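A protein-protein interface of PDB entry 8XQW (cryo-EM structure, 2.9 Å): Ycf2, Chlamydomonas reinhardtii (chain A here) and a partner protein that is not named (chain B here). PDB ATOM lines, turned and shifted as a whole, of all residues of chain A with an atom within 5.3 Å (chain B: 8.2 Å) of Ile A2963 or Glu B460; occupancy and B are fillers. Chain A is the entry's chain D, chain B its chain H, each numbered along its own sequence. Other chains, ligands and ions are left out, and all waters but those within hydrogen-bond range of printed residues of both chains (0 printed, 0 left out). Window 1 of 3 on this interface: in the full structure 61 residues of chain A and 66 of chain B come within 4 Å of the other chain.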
ATOM      1  N   LYS A2930     -20.477 -24.631  21.899  1.00  0.00           N
ATOM      2  CA  LYS A2930     -19.024 -24.450  21.918  1.00  0.00           C
ATOM      3  C   LYS A2930     -18.611 -23.105  21.334  1.00  0.00           C
ATOM      4  O   LYS A2930     -17.767 -22.404  21.903  1.00  0.00           O
ATOM      5  CB  LYS A2930     -18.343 -25.577  21.162  1.00  0.00           C
ATOM      6  CG  LYS A2930     -18.794 -26.932  21.585  1.00  0.00           C
ATOM      7  CD  LYS A2930     -17.639 -27.805  21.982  1.00  0.00           C
ATOM      8  CE  LYS A2930     -17.206 -27.511  23.391  1.00  0.00           C
ATOM      9  NZ  LYS A2930     -16.239 -28.524  23.871  1.00  0.00           N
ATOM     10  N   PHE A2931     -19.176 -22.729  20.189  1.00  0.00           N
ATOM     11  CA  PHE A2931     -18.805 -21.461  19.576  1.00  0.00           C
ATOM     12  C   PHE A2931     -19.139 -20.285  20.467  1.00  0.00           C
ATOM     13  O   PHE A2931     -18.419 -19.289  20.461  1.00  0.00           O
ATOM     14  CB  PHE A2931     -19.509 -21.277  18.244  1.00  0.00           C
ATOM     15  CG  PHE A2931     -18.805 -21.901  17.095  1.00  0.00           C
ATOM     16  CD1 PHE A2931     -18.038 -23.024  17.270  1.00  0.00           C
ATOM     17  CD2 PHE A2931     -18.919 -21.371  15.835  1.00  0.00           C
ATOM     18  CE1 PHE A2931     -17.403 -23.603  16.219  1.00  0.00           C
ATOM     19  CE2 PHE A2931     -18.285 -21.948  14.782  1.00  0.00           C
ATOM     20  CZ  PHE A2931     -17.527 -23.065  14.973  1.00  0.00           C
ATOM     21  N   LEU A2934     -16.460 -20.033  23.185  1.00  0.00           N
ATOM     22  CA  LEU A2934     -15.119 -19.640  22.751  1.00  0.00           C
ATOM     23  C   LEU A2934     -14.978 -18.129  22.640  1.00  0.00           C
ATOM     24  O   LEU A2934     -14.087 -17.540  23.250  1.00  0.00           O
ATOM     25  CB  LEU A2934     -14.763 -20.277  21.413  1.00  0.00           C
ATOM     26  CG  LEU A2934     -14.410 -21.754  21.380  1.00  0.00           C
ATOM     27  CD1 LEU A2934     -13.786 -22.070  20.053  1.00  0.00           C
ATOM     28  CD2 LEU A2934     -13.479 -22.110  22.504  1.00  0.00           C
ATOM     29  N   SER A2958      -8.279 -21.933  13.960  1.00  0.00           N
ATOM     30  CA  SER A2958      -7.771 -23.296  14.042  1.00  0.00           C
ATOM     31  C   SER A2958      -8.347 -24.055  15.230  1.00  0.00           C
ATOM     32  O   SER A2958      -8.623 -25.257  15.125  1.00  0.00           O
ATOM     33  CB  SER A2958      -6.254 -23.266  14.095  1.00  0.00           C
ATOM     34  OG  SER A2958      -5.769 -22.238  13.253  1.00  0.00           O
ATOM     35  N   THR A2959      -8.554 -23.380  16.358  1.00  0.00           N
ATOM     36  CA  THR A2959      -9.284 -24.009  17.448  1.00  0.00           C
ATOM     37  C   THR A2959     -10.691 -24.385  17.011  1.00  0.00           C
ATOM     38  O   THR A2959     -11.168 -25.493  17.297  1.00  0.00           O
ATOM     39  CB  THR A2959      -9.342 -23.078  18.647  1.00  0.00           C
ATOM     40  OG1 THR A2959      -8.047 -22.514  18.868  1.00  0.00           O
ATOM     41  CG2 THR A2959      -9.767 -23.842  19.870  1.00  0.00           C
ATOM     42  N   LYS A2960     -11.363 -23.486  16.299  1.00  0.00           N
ATOM     43  CA  LYS A2960     -12.711 -23.775  15.843  1.00  0.00           C
ATOM     44  C   LYS A2960     -12.723 -24.891  14.817  1.00  0.00           C
ATOM     45  O   LYS A2960     -13.707 -25.624  14.716  1.00  0.00           O
ATOM     46  CB  LYS A2960     -13.340 -22.512  15.286  1.00  0.00           C
ATOM     47  CG  LYS A2960     -13.527 -21.458  16.338  1.00  0.00           C
ATOM     48  CD  LYS A2960     -14.256 -20.257  15.803  1.00  0.00           C
ATOM     49  CE  LYS A2960     -14.746 -19.391  16.940  1.00  0.00           C
ATOM     50  NZ  LYS A2960     -15.690 -18.339  16.478  1.00  0.00           N
ATOM     51  N   GLU A2961     -11.629 -25.079  14.088  1.00  0.00           N
ATOM     52  CA  GLU A2961     -11.594 -26.195  13.157  1.00  0.00           C
ATOM     53  C   GLU A2961     -11.416 -27.521  13.877  1.00  0.00           C
ATOM     54  O   GLU A2961     -12.046 -28.519  13.503  1.00  0.00           O
ATOM     55  CB  GLU A2961     -10.488 -26.000  12.136  1.00  0.00           C
ATOM     56  CG  GLU A2961     -10.349 -27.179  11.215  1.00  0.00           C
ATOM     57  CD  GLU A2961      -9.349 -26.941  10.108  1.00  0.00           C
ATOM     58  OE1 GLU A2961      -8.326 -26.273  10.365  1.00  0.00           O
ATOM     59  OE2 GLU A2961      -9.588 -27.423   8.981  1.00  0.00           O
ATOM     60  N   ILE A2962     -10.571 -27.561  14.906  1.00  0.00           N
ATOM     61  CA  ILE A2962     -10.503 -28.766  15.732  1.00  0.00           C
ATOM     62  C   ILE A2962     -11.883 -29.104  16.266  1.00  0.00           C
ATOM     63  O   ILE A2962     -12.325 -30.262  16.240  1.00  0.00           O
ATOM     64  CB  ILE A2962      -9.503 -28.583  16.885  1.00  0.00           C
ATOM     65  CG1 ILE A2962      -8.182 -28.015  16.381  1.00  0.00           C
ATOM     66  CG2 ILE A2962      -9.283 -29.888  17.583  1.00  0.00           C
ATOM     67  CD1 ILE A2962      -7.432 -28.935  15.500  1.00  0.00           C
ATOM     68  N   ILE A2963     -12.587 -28.088  16.754  1.00  0.00           N
ATOM     69  CA  ILE A2963     -13.873 -28.325  17.394  1.00  0.00           C
ATOM     70  C   ILE A2963     -14.903 -28.826  16.392  1.00  0.00           C
ATOM     71  O   ILE A2963     -15.680 -29.739  16.688  1.00  0.00           O
ATOM     72  CB  ILE A2963     -14.329 -27.047  18.102  1.00  0.00           C
ATOM     73  CG1 ILE A2963     -13.647 -26.953  19.456  1.00  0.00           C
ATOM     74  CG2 ILE A2963     -15.827 -27.021  18.244  1.00  0.00           C
ATOM     75  CD1 ILE A2963     -13.973 -25.709  20.195  1.00  0.00           C
ATOM     76  N   LEU A2964     -14.926 -28.251  15.192  1.00  0.00           N
ATOM     77  CA  LEU A2964     -15.888 -28.687  14.189  1.00  0.00           C
ATOM     78  C   LEU A2964     -15.615 -30.115  13.741  1.00  0.00           C
ATOM     79  O   LEU A2964     -16.548 -30.908  13.583  1.00  0.00           O
ATOM     80  CB  LEU A2964     -15.856 -27.745  12.996  1.00  0.00           C
ATOM     81  CG  LEU A2964     -17.164 -27.605  12.232  1.00  0.00           C
ATOM     82  CD1 LEU A2964     -17.930 -26.441  12.767  1.00  0.00           C
ATOM     83  CD2 LEU A2964     -16.891 -27.412  10.779  1.00  0.00           C
ATOM     84  N   THR A2965     -14.349 -30.463  13.525  1.00  0.00           N
ATOM     85  CA  THR A2965     -14.028 -31.827  13.121  1.00  0.00           C
ATOM     86  C   THR A2965     -14.440 -32.829  14.188  1.00  0.00           C
ATOM     87  O   THR A2965     -15.034 -33.874  13.886  1.00  0.00           O
ATOM     88  CB  THR A2965     -12.542 -31.943  12.832  1.00  0.00           C
ATOM     89  OG1 THR A2965     -12.127 -30.833  12.037  1.00  0.00           O
ATOM     90  CG2 THR A2965     -12.263 -33.209  12.085  1.00  0.00           C
ATOM     91  N   ASN A2966     -14.152 -32.523  15.452  1.00  0.00           N
ATOM     92  CA  ASN A2966     -14.550 -33.436  16.516  1.00  0.00           C
ATOM     93  C   ASN A2966     -16.057 -33.573  16.597  1.00  0.00           C
ATOM     94  O   ASN A2966     -16.575 -34.683  16.721  1.00  0.00           O
ATOM     95  CB  ASN A2966     -14.010 -32.963  17.848  1.00  0.00           C
ATOM     96  CG  ASN A2966     -12.583 -33.293  18.022  1.00  0.00           C
ATOM     97  OD1 ASN A2966     -11.915 -33.691  17.080  1.00  0.00           O
ATOM     98  ND2 ASN A2966     -12.086 -33.125  19.228  1.00  0.00           N
ATOM     99  N   SER A2967     -16.780 -32.456  16.554  1.00  0.00           N
ATOM    100  CA  SER A2967     -18.230 -32.528  16.650  1.00  0.00           C
ATOM    101  C   SER A2967     -18.818 -33.325  15.504  1.00  0.00           C
ATOM    102  O   SER A2967     -19.830 -34.005  15.672  1.00  0.00           O
ATOM    103  CB  SER A2967     -18.819 -31.128  16.679  1.00  0.00           C
ATOM    104  OG  SER A2967     -18.300 -30.398  17.769  1.00  0.00           O
ATOM    105  N   PHE A2968     -18.207 -33.259  14.330  1.00  0.00           N
ATOM    106  CA  PHE A2968     -18.704 -34.080  13.240  1.00  0.00           C
ATOM    107  C   PHE A2968     -18.406 -35.545  13.470  1.00  0.00           C
ATOM    108  O   PHE A2968     -19.160 -36.409  13.023  1.00  0.00           O
ATOM    109  CB  PHE A2968     -18.100 -33.629  11.924  1.00  0.00           C
ATOM    110  CG  PHE A2968     -19.080 -32.995  11.014  1.00  0.00           C
ATOM    111  CD1 PHE A2968     -19.855 -33.763  10.183  1.00  0.00           C
ATOM    112  CD2 PHE A2968     -19.244 -31.633  11.003  1.00  0.00           C
ATOM    113  CE1 PHE A2968     -20.761 -33.185   9.357  1.00  0.00           C
ATOM    114  CE2 PHE A2968     -20.149 -31.056  10.174  1.00  0.00           C
ATOM    115  CZ  PHE A2968     -20.909 -31.834   9.353  1.00  0.00           C
ATOM    116  N   ARG A2970     -18.276 -37.039  16.509  1.00  0.00           N
ATOM    117  CA  ARG A2970     -19.099 -37.554  17.598  1.00  0.00           C
ATOM    118  C   ARG A2970     -20.562 -37.643  17.201  1.00  0.00           C
ATOM    119  O   ARG A2970     -21.137 -38.731  17.155  1.00  0.00           O
ATOM    120  CB  ARG A2970     -18.962 -36.668  18.827  1.00  0.00           C
ATOM    121  CG  ARG A2970     -17.665 -36.811  19.529  1.00  0.00           C
ATOM    122  CD  ARG A2970     -17.157 -35.475  19.935  1.00  0.00           C
ATOM    123  NE  ARG A2970     -17.627 -35.107  21.253  1.00  0.00           N
ATOM    124  CZ  ARG A2970     -17.282 -33.989  21.865  1.00  0.00           C
ATOM    125  NH1 ARG A2970     -16.478 -33.136  21.269  1.00  0.00           N
ATOM    126  NH2 ARG A2970     -17.749 -33.720  23.066  1.00  0.00           N
ATOM    127  N   ASP B 196     -18.925 -32.530  28.554  1.00  0.00           N
ATOM    128  CA  ASP B 196     -18.760 -32.107  27.170  1.00  0.00           C
ATOM    129  C   ASP B 196     -17.571 -32.763  26.490  1.00  0.00           C
ATOM    130  O   ASP B 196     -17.521 -32.806  25.256  1.00  0.00           O
ATOM    131  CB  ASP B 196     -18.615 -30.600  27.086  1.00  0.00           C
ATOM    132  CG  ASP B 196     -17.273 -30.136  27.531  1.00  0.00           C
ATOM    133  OD1 ASP B 196     -16.770 -30.681  28.529  1.00  0.00           O
ATOM    134  OD2 ASP B 196     -16.708 -29.240  26.877  1.00  0.00           O
ATOM    135  N   THR B 197     -16.605 -33.269  27.246  1.00  0.00           N
ATOM    136  CA  THR B 197     -15.426 -33.827  26.604  1.00  0.00           C
ATOM    137  C   THR B 197     -15.616 -35.259  26.144  1.00  0.00           C
ATOM    138  O   THR B 197     -14.759 -35.772  25.426  1.00  0.00           O
ATOM    139  CB  THR B 197     -14.223 -33.761  27.537  1.00  0.00           C
ATOM    140  OG1 THR B 197     -14.639 -34.041  28.876  1.00  0.00           O
ATOM    141  CG2 THR B 197     -13.599 -32.389  27.487  1.00  0.00           C
ATOM    142  N   PHE B 455     -16.190 -41.317  22.352  1.00  0.00           N
ATOM    143  CA  PHE B 455     -15.078 -40.650  21.696  1.00  0.00           C
ATOM    144  C   PHE B 455     -14.516 -39.623  22.651  1.00  0.00           C
ATOM    145  O   PHE B 455     -15.124 -38.572  22.853  1.00  0.00           O
ATOM    146  CB  PHE B 455     -15.531 -39.985  20.401  1.00  0.00           C
ATOM    147  CG  PHE B 455     -14.460 -39.210  19.716  1.00  0.00           C
ATOM    148  CD1 PHE B 455     -13.495 -39.852  18.980  1.00  0.00           C
ATOM    149  CD2 PHE B 455     -14.413 -37.840  19.811  1.00  0.00           C
ATOM    150  CE1 PHE B 455     -12.508 -39.141  18.358  1.00  0.00           C
ATOM    151  CE2 PHE B 455     -13.431 -37.129  19.185  1.00  0.00           C
ATOM    152  CZ  PHE B 455     -12.479 -37.777  18.461  1.00  0.00           C
ATOM    153  N   ASP B 456     -13.360 -39.914  23.230  1.00  0.00           N
ATOM    154  CA  ASP B 456     -12.754 -39.021  24.202  1.00  0.00           C
ATOM    155  C   ASP B 456     -11.956 -37.960  23.467  1.00  0.00           C
ATOM    156  O   ASP B 456     -10.948 -38.268  22.827  1.00  0.00           O
ATOM    157  CB  ASP B 456     -11.858 -39.781  25.168  1.00  0.00           C
ATOM    158  CG  ASP B 456     -11.456 -38.940  26.353  1.00  0.00           C
ATOM    159  OD1 ASP B 456     -12.283 -38.770  27.267  1.00  0.00           O
ATOM    160  OD2 ASP B 456     -10.320 -38.430  26.365  1.00  0.00           O
ATOM    161  N   ALA B 457     -12.392 -36.716  23.575  1.00  0.00           N
ATOM    162  CA  ALA B 457     -11.788 -35.599  22.877  1.00  0.00           C
ATOM    163  C   ALA B 457     -11.218 -34.603  23.865  1.00  0.00           C
ATOM    164  O   ALA B 457     -11.415 -33.397  23.743  1.00  0.00           O
ATOM    165  CB  ALA B 457     -12.796 -34.924  21.961  1.00  0.00           C
ATOM    166  N   SER B 458     -10.512 -35.106  24.871  1.00  0.00           N
ATOM    167  CA  SER B 458      -9.945 -34.226  25.879  1.00  0.00           C
ATOM    168  C   SER B 458      -8.778 -33.417  25.354  1.00  0.00           C
ATOM    169  O   SER B 458      -8.500 -32.344  25.892  1.00  0.00           O
ATOM    170  CB  SER B 458      -9.509 -35.037  27.091  1.00  0.00           C
ATOM    171  OG  SER B 458      -9.084 -36.322  26.695  1.00  0.00           O
ATOM    172  N   PHE B 459      -8.103 -33.886  24.307  1.00  0.00           N
ATOM    173  CA  PHE B 459      -6.967 -33.141  23.787  1.00  0.00           C
ATOM    174  C   PHE B 459      -7.349 -31.739  23.360  1.00  0.00           C
ATOM    175  O   PHE B 459      -6.475 -30.873  23.281  1.00  0.00           O
ATOM    176  CB  PHE B 459      -6.327 -33.885  22.622  1.00  0.00           C
ATOM    177  CG  PHE B 459      -7.229 -34.073  21.448  1.00  0.00           C
ATOM    178  CD1 PHE B 459      -7.333 -33.107  20.475  1.00  0.00           C
ATOM    179  CD2 PHE B 459      -7.951 -35.231  21.300  1.00  0.00           C
ATOM    180  CE1 PHE B 459      -8.153 -33.284  19.400  1.00  0.00           C
ATOM    181  CE2 PHE B 459      -8.768 -35.410  20.221  1.00  0.00           C
ATOM    182  CZ  PHE B 459      -8.870 -34.436  19.274  1.00  0.00           C
ATOM    183  N   GLU B 460      -8.631 -31.491  23.101  1.00  0.00           N
ATOM    184  CA  GLU B 460      -9.075 -30.151  22.747  1.00  0.00           C
ATOM    185  C   GLU B 460      -8.694 -29.146  23.813  1.00  0.00           C
ATOM    186  O   GLU B 460      -8.323 -28.010  23.500  1.00  0.00           O
ATOM    187  CB  GLU B 460     -10.577 -30.138  22.557  1.00  0.00           C
ATOM    188  CG  GLU B 460     -11.033 -30.488  21.185  1.00  0.00           C
ATOM    189  CD  GLU B 460     -12.539 -30.555  21.114  1.00  0.00           C
ATOM    190  OE1 GLU B 460     -13.200 -29.938  21.975  1.00  0.00           O
ATOM    191  OE2 GLU B 460     -13.070 -31.231  20.211  1.00  0.00           O
ATOM    192  N   LYS B 461      -8.770 -29.547  25.080  1.00  0.00           N
ATOM    193  CA  LYS B 461      -8.434 -28.629  26.157  1.00  0.00           C
ATOM    194  C   LYS B 461      -7.023 -28.097  26.017  1.00  0.00           C
ATOM    195  O   LYS B 461      -6.733 -26.989  26.471  1.00  0.00           O
ATOM    196  CB  LYS B 461      -8.604 -29.319  27.500  1.00  0.00           C
ATOM    197  CG  LYS B 461      -9.984 -29.205  28.053  1.00  0.00           C
ATOM    198  CD  LYS B 461     -10.079 -29.902  29.372  1.00  0.00           C
ATOM    199  CE  LYS B 461      -9.889 -31.378  29.188  1.00  0.00           C
ATOM    200  NZ  LYS B 461     -10.260 -32.135  30.406  1.00  0.00           N
ATOM    201  N   LEU B 462      -6.133 -28.858  25.387  1.00  0.00           N
ATOM    202  CA  LEU B 462      -4.791 -28.353  25.142  1.00  0.00           C
ATOM    203  C   LEU B 462      -4.830 -27.168  24.201  1.00  0.00           C
ATOM    204  O   LEU B 462      -4.317 -26.092  24.519  1.00  0.00           O
ATOM    205  CB  LEU B 462      -3.916 -29.457  24.569  1.00  0.00           C
ATOM    206  CG  LEU B 462      -2.935 -30.076  25.547  1.00  0.00           C
ATOM    207  CD1 LEU B 462      -2.331 -31.303  24.945  1.00  0.00           C
ATOM    208  CD2 LEU B 462      -1.866 -29.080  25.871  1.00  0.00           C
ATOM    209  N   TYR B 463      -5.480 -27.333  23.053  1.00  0.00           N
ATOM    210  CA  TYR B 463      -5.493 -26.280  22.049  1.00  0.00           C
ATOM    211  C   TYR B 463      -6.011 -24.978  22.630  1.00  0.00           C
ATOM    212  O   TYR B 463      -5.330 -23.951  22.570  1.00  0.00           O
ATOM    213  CB  TYR B 463      -6.331 -26.716  20.863  1.00  0.00           C
ATOM    214  CG  TYR B 463      -5.596 -27.653  19.958  1.00  0.00           C
ATOM    215  CD1 TYR B 463      -5.584 -29.005  20.197  1.00  0.00           C
ATOM    216  CD2 TYR B 463      -4.910 -27.181  18.867  1.00  0.00           C
ATOM    217  CE1 TYR B 463      -4.923 -29.856  19.374  1.00  0.00           C
ATOM    218  CE2 TYR B 463      -4.235 -28.022  18.045  1.00  0.00           C
ATOM    219  CZ  TYR B 463      -4.244 -29.359  18.300  1.00  0.00           C
ATOM    220  OH  TYR B 463      -3.569 -30.204  17.462  1.00  0.00           O
ATOM    221  N   THR B 464      -7.191 -25.014  23.244  1.00  0.00           N
ATOM    222  CA  THR B 464      -7.721 -23.811  23.869  1.00  0.00           C
ATOM    223  C   THR B 464      -6.717 -23.209  24.837  1.00  0.00           C
ATOM    224  O   THR B 464      -6.454 -22.004  24.790  1.00  0.00           O
ATOM    225  CB  THR B 464      -9.030 -24.113  24.581  1.00  0.00           C
ATOM    226  OG1 THR B 464      -8.761 -24.861  25.765  1.00  0.00           O
ATOM    227  CG2 THR B 464      -9.929 -24.917  23.692  1.00  0.00           C
ATOM    228  N   TYR B 465      -6.109 -24.034  25.686  1.00  0.00           N
ATOM    229  CA  TYR B 465      -5.101 -23.512  26.598  1.00  0.00           C
ATOM    230  C   TYR B 465      -4.034 -22.741  25.841  1.00  0.00           C
ATOM    231  O   TYR B 465      -3.793 -21.560  26.106  1.00  0.00           O
ATOM    232  CB  TYR B 465      -4.475 -24.650  27.389  1.00  0.00           C
ATOM    233  CG  TYR B 465      -3.400 -24.205  28.335  1.00  0.00           C
ATOM    234  CD1 TYR B 465      -3.716 -23.630  29.543  1.00  0.00           C
ATOM    235  CD2 TYR B 465      -2.070 -24.369  28.026  1.00  0.00           C
ATOM    236  CE1 TYR B 465      -2.740 -23.225  30.406  1.00  0.00           C
ATOM    237  CE2 TYR B 465      -1.092 -23.965  28.883  1.00  0.00           C
ATOM    238  CZ  TYR B 465      -1.432 -23.393  30.068  1.00  0.00           C
ATOM    239  OH  TYR B 465      -0.452 -22.987  30.931  1.00  0.00           O
ATOM    240  N   PHE B 466      -3.444 -23.364  24.840  1.00  0.00           N
ATOM    241  CA  PHE B 466      -2.324 -22.718  24.189  1.00  0.00           C
ATOM    242  C   PHE B 466      -2.737 -21.593  23.271  1.00  0.00           C
ATOM    243  O   PHE B 466      -1.876 -21.032  22.596  1.00  0.00           O
ATOM    244  CB  PHE B 466      -1.502 -23.741  23.420  1.00  0.00           C
ATOM    245  CG  PHE B 466      -0.479 -24.403  24.257  1.00  0.00           C
ATOM    246  CD1 PHE B 466       0.689 -23.765  24.563  1.00  0.00           C
ATOM    247  CD2 PHE B 466      -0.701 -25.648  24.772  1.00  0.00           C
ATOM    248  CE1 PHE B 466       1.604 -24.362  25.346  1.00  0.00           C
ATOM    249  CE2 PHE B 466       0.214 -26.236  25.556  1.00  0.00           C
ATOM    250  CZ  PHE B 466       1.366 -25.595  25.842  1.00  0.00           C
ATOM    251  N   ASP B 467      -4.014 -21.233  23.215  1.00  0.00           N
ATOM    252  CA  ASP B 467      -4.300 -20.029  22.457  1.00  0.00           C
ATOM    253  C   ASP B 467      -4.443 -18.817  23.353  1.00  0.00           C
ATOM    254  O   ASP B 467      -4.516 -17.700  22.844  1.00  0.00           O
ATOM    255  CB  ASP B 467      -5.534 -20.227  21.570  1.00  0.00           C
ATOM    256  CG  ASP B 467      -6.844 -20.192  22.327  1.00  0.00           C
ATOM    257  OD1 ASP B 467      -6.888 -19.816  23.514  1.00  0.00           O
ATOM    258  OD2 ASP B 467      -7.868 -20.549  21.712  1.00  0.00           O
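Of chain B, only Glu B460 comes within 4 Å of Ile A2963.
Of chain A, only Lys A2930, Ile A2963 and Asn A2966 come within 4 Å of Glu B460.
Of the printed residues of chain B, Lys A2930 touches Asp B196 (3.1 Å) and Glu B460 (3.9 Å).
Of the printed residues of chain A, Asp B196 touches Lys A2930 (3.1 Å) and Arg A2970 (2.4 Å).
Of the printed residues of chain A, Asp B467 touches Thr A2959.
Ser A2967 touches none of the printed residues of chain B.
The nearest residue of chain B that does not touch Ile A2963 is Thr B464 (5.4 Å).
The side-chain amino group of Lys A2930 is in salt-bridge range of the side-chain carboxylate of Asp B196 (3.1 Å).
NZ of Lys A2930 lies within salt-bridge range of OE1 of Glu B460, at 3.9 Å.
The side-chain carboxylate (OD2) of Asp B467 lies within hydrogen-bond range of the side-chain hydroxyl (OG1) of Thr A2959 (3.5 Å).
The side-chain carboxylate (OE2) of Glu B460 sits close to the side-chain amide nitrogen (ND2) of Asn A2966 (2.3 Å).
O of Asp B196 lies close to NH2 of Arg A2970, at 2.4 Å.
Of the 15 printed residues of chain B, 7 touch a printed residue of chain A.
Along chain B the printed residues that touch a printed residue of chain A span positions 196 to 467.
Among the printed residues, 10 pairs touch across the chains.
Among the printed residues, Asp or Glu carboxylates within 4 Å of a Lys or Arg side-chain nitrogen of the other chain: Lys A2930 with Asp B196 and Lys A2930 with Glu B460.
The side-chain hydroxyl (OG) of Ser A2967 lies within hydrogen-bond range of the backbone carbonyl oxygen (O) of Ile A2963 (2.9 Å).
The backbone carbonyl oxygen (O) of Thr B197 lies within hydrogen-bond range of the backbone NH (N) of Ala B457 (3.1 Å).
The backbone carbonyl oxygen (O) of Lys B461 sits at hydrogen-bond distance from the side-chain hydroxyl (OG1) of Thr B464 (3.0 Å).
The backbone carbonyl oxygen (O) of Thr B464 sits close to the side-chain carboxylate (OD1) of Asp B467, at 2.6 Å.
Among the printed residues, merely in contact across the chains: Thr A2959 with Thr B464 (3.97 Å), Ile A2963 with Glu B460 (3.9 Å), Asn A2966 with Ala B457 (3.3 Å), Asn A2966 with Phe B459 (3.5 Å) and Arg A2970 with Phe B455 (3.4 Å).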
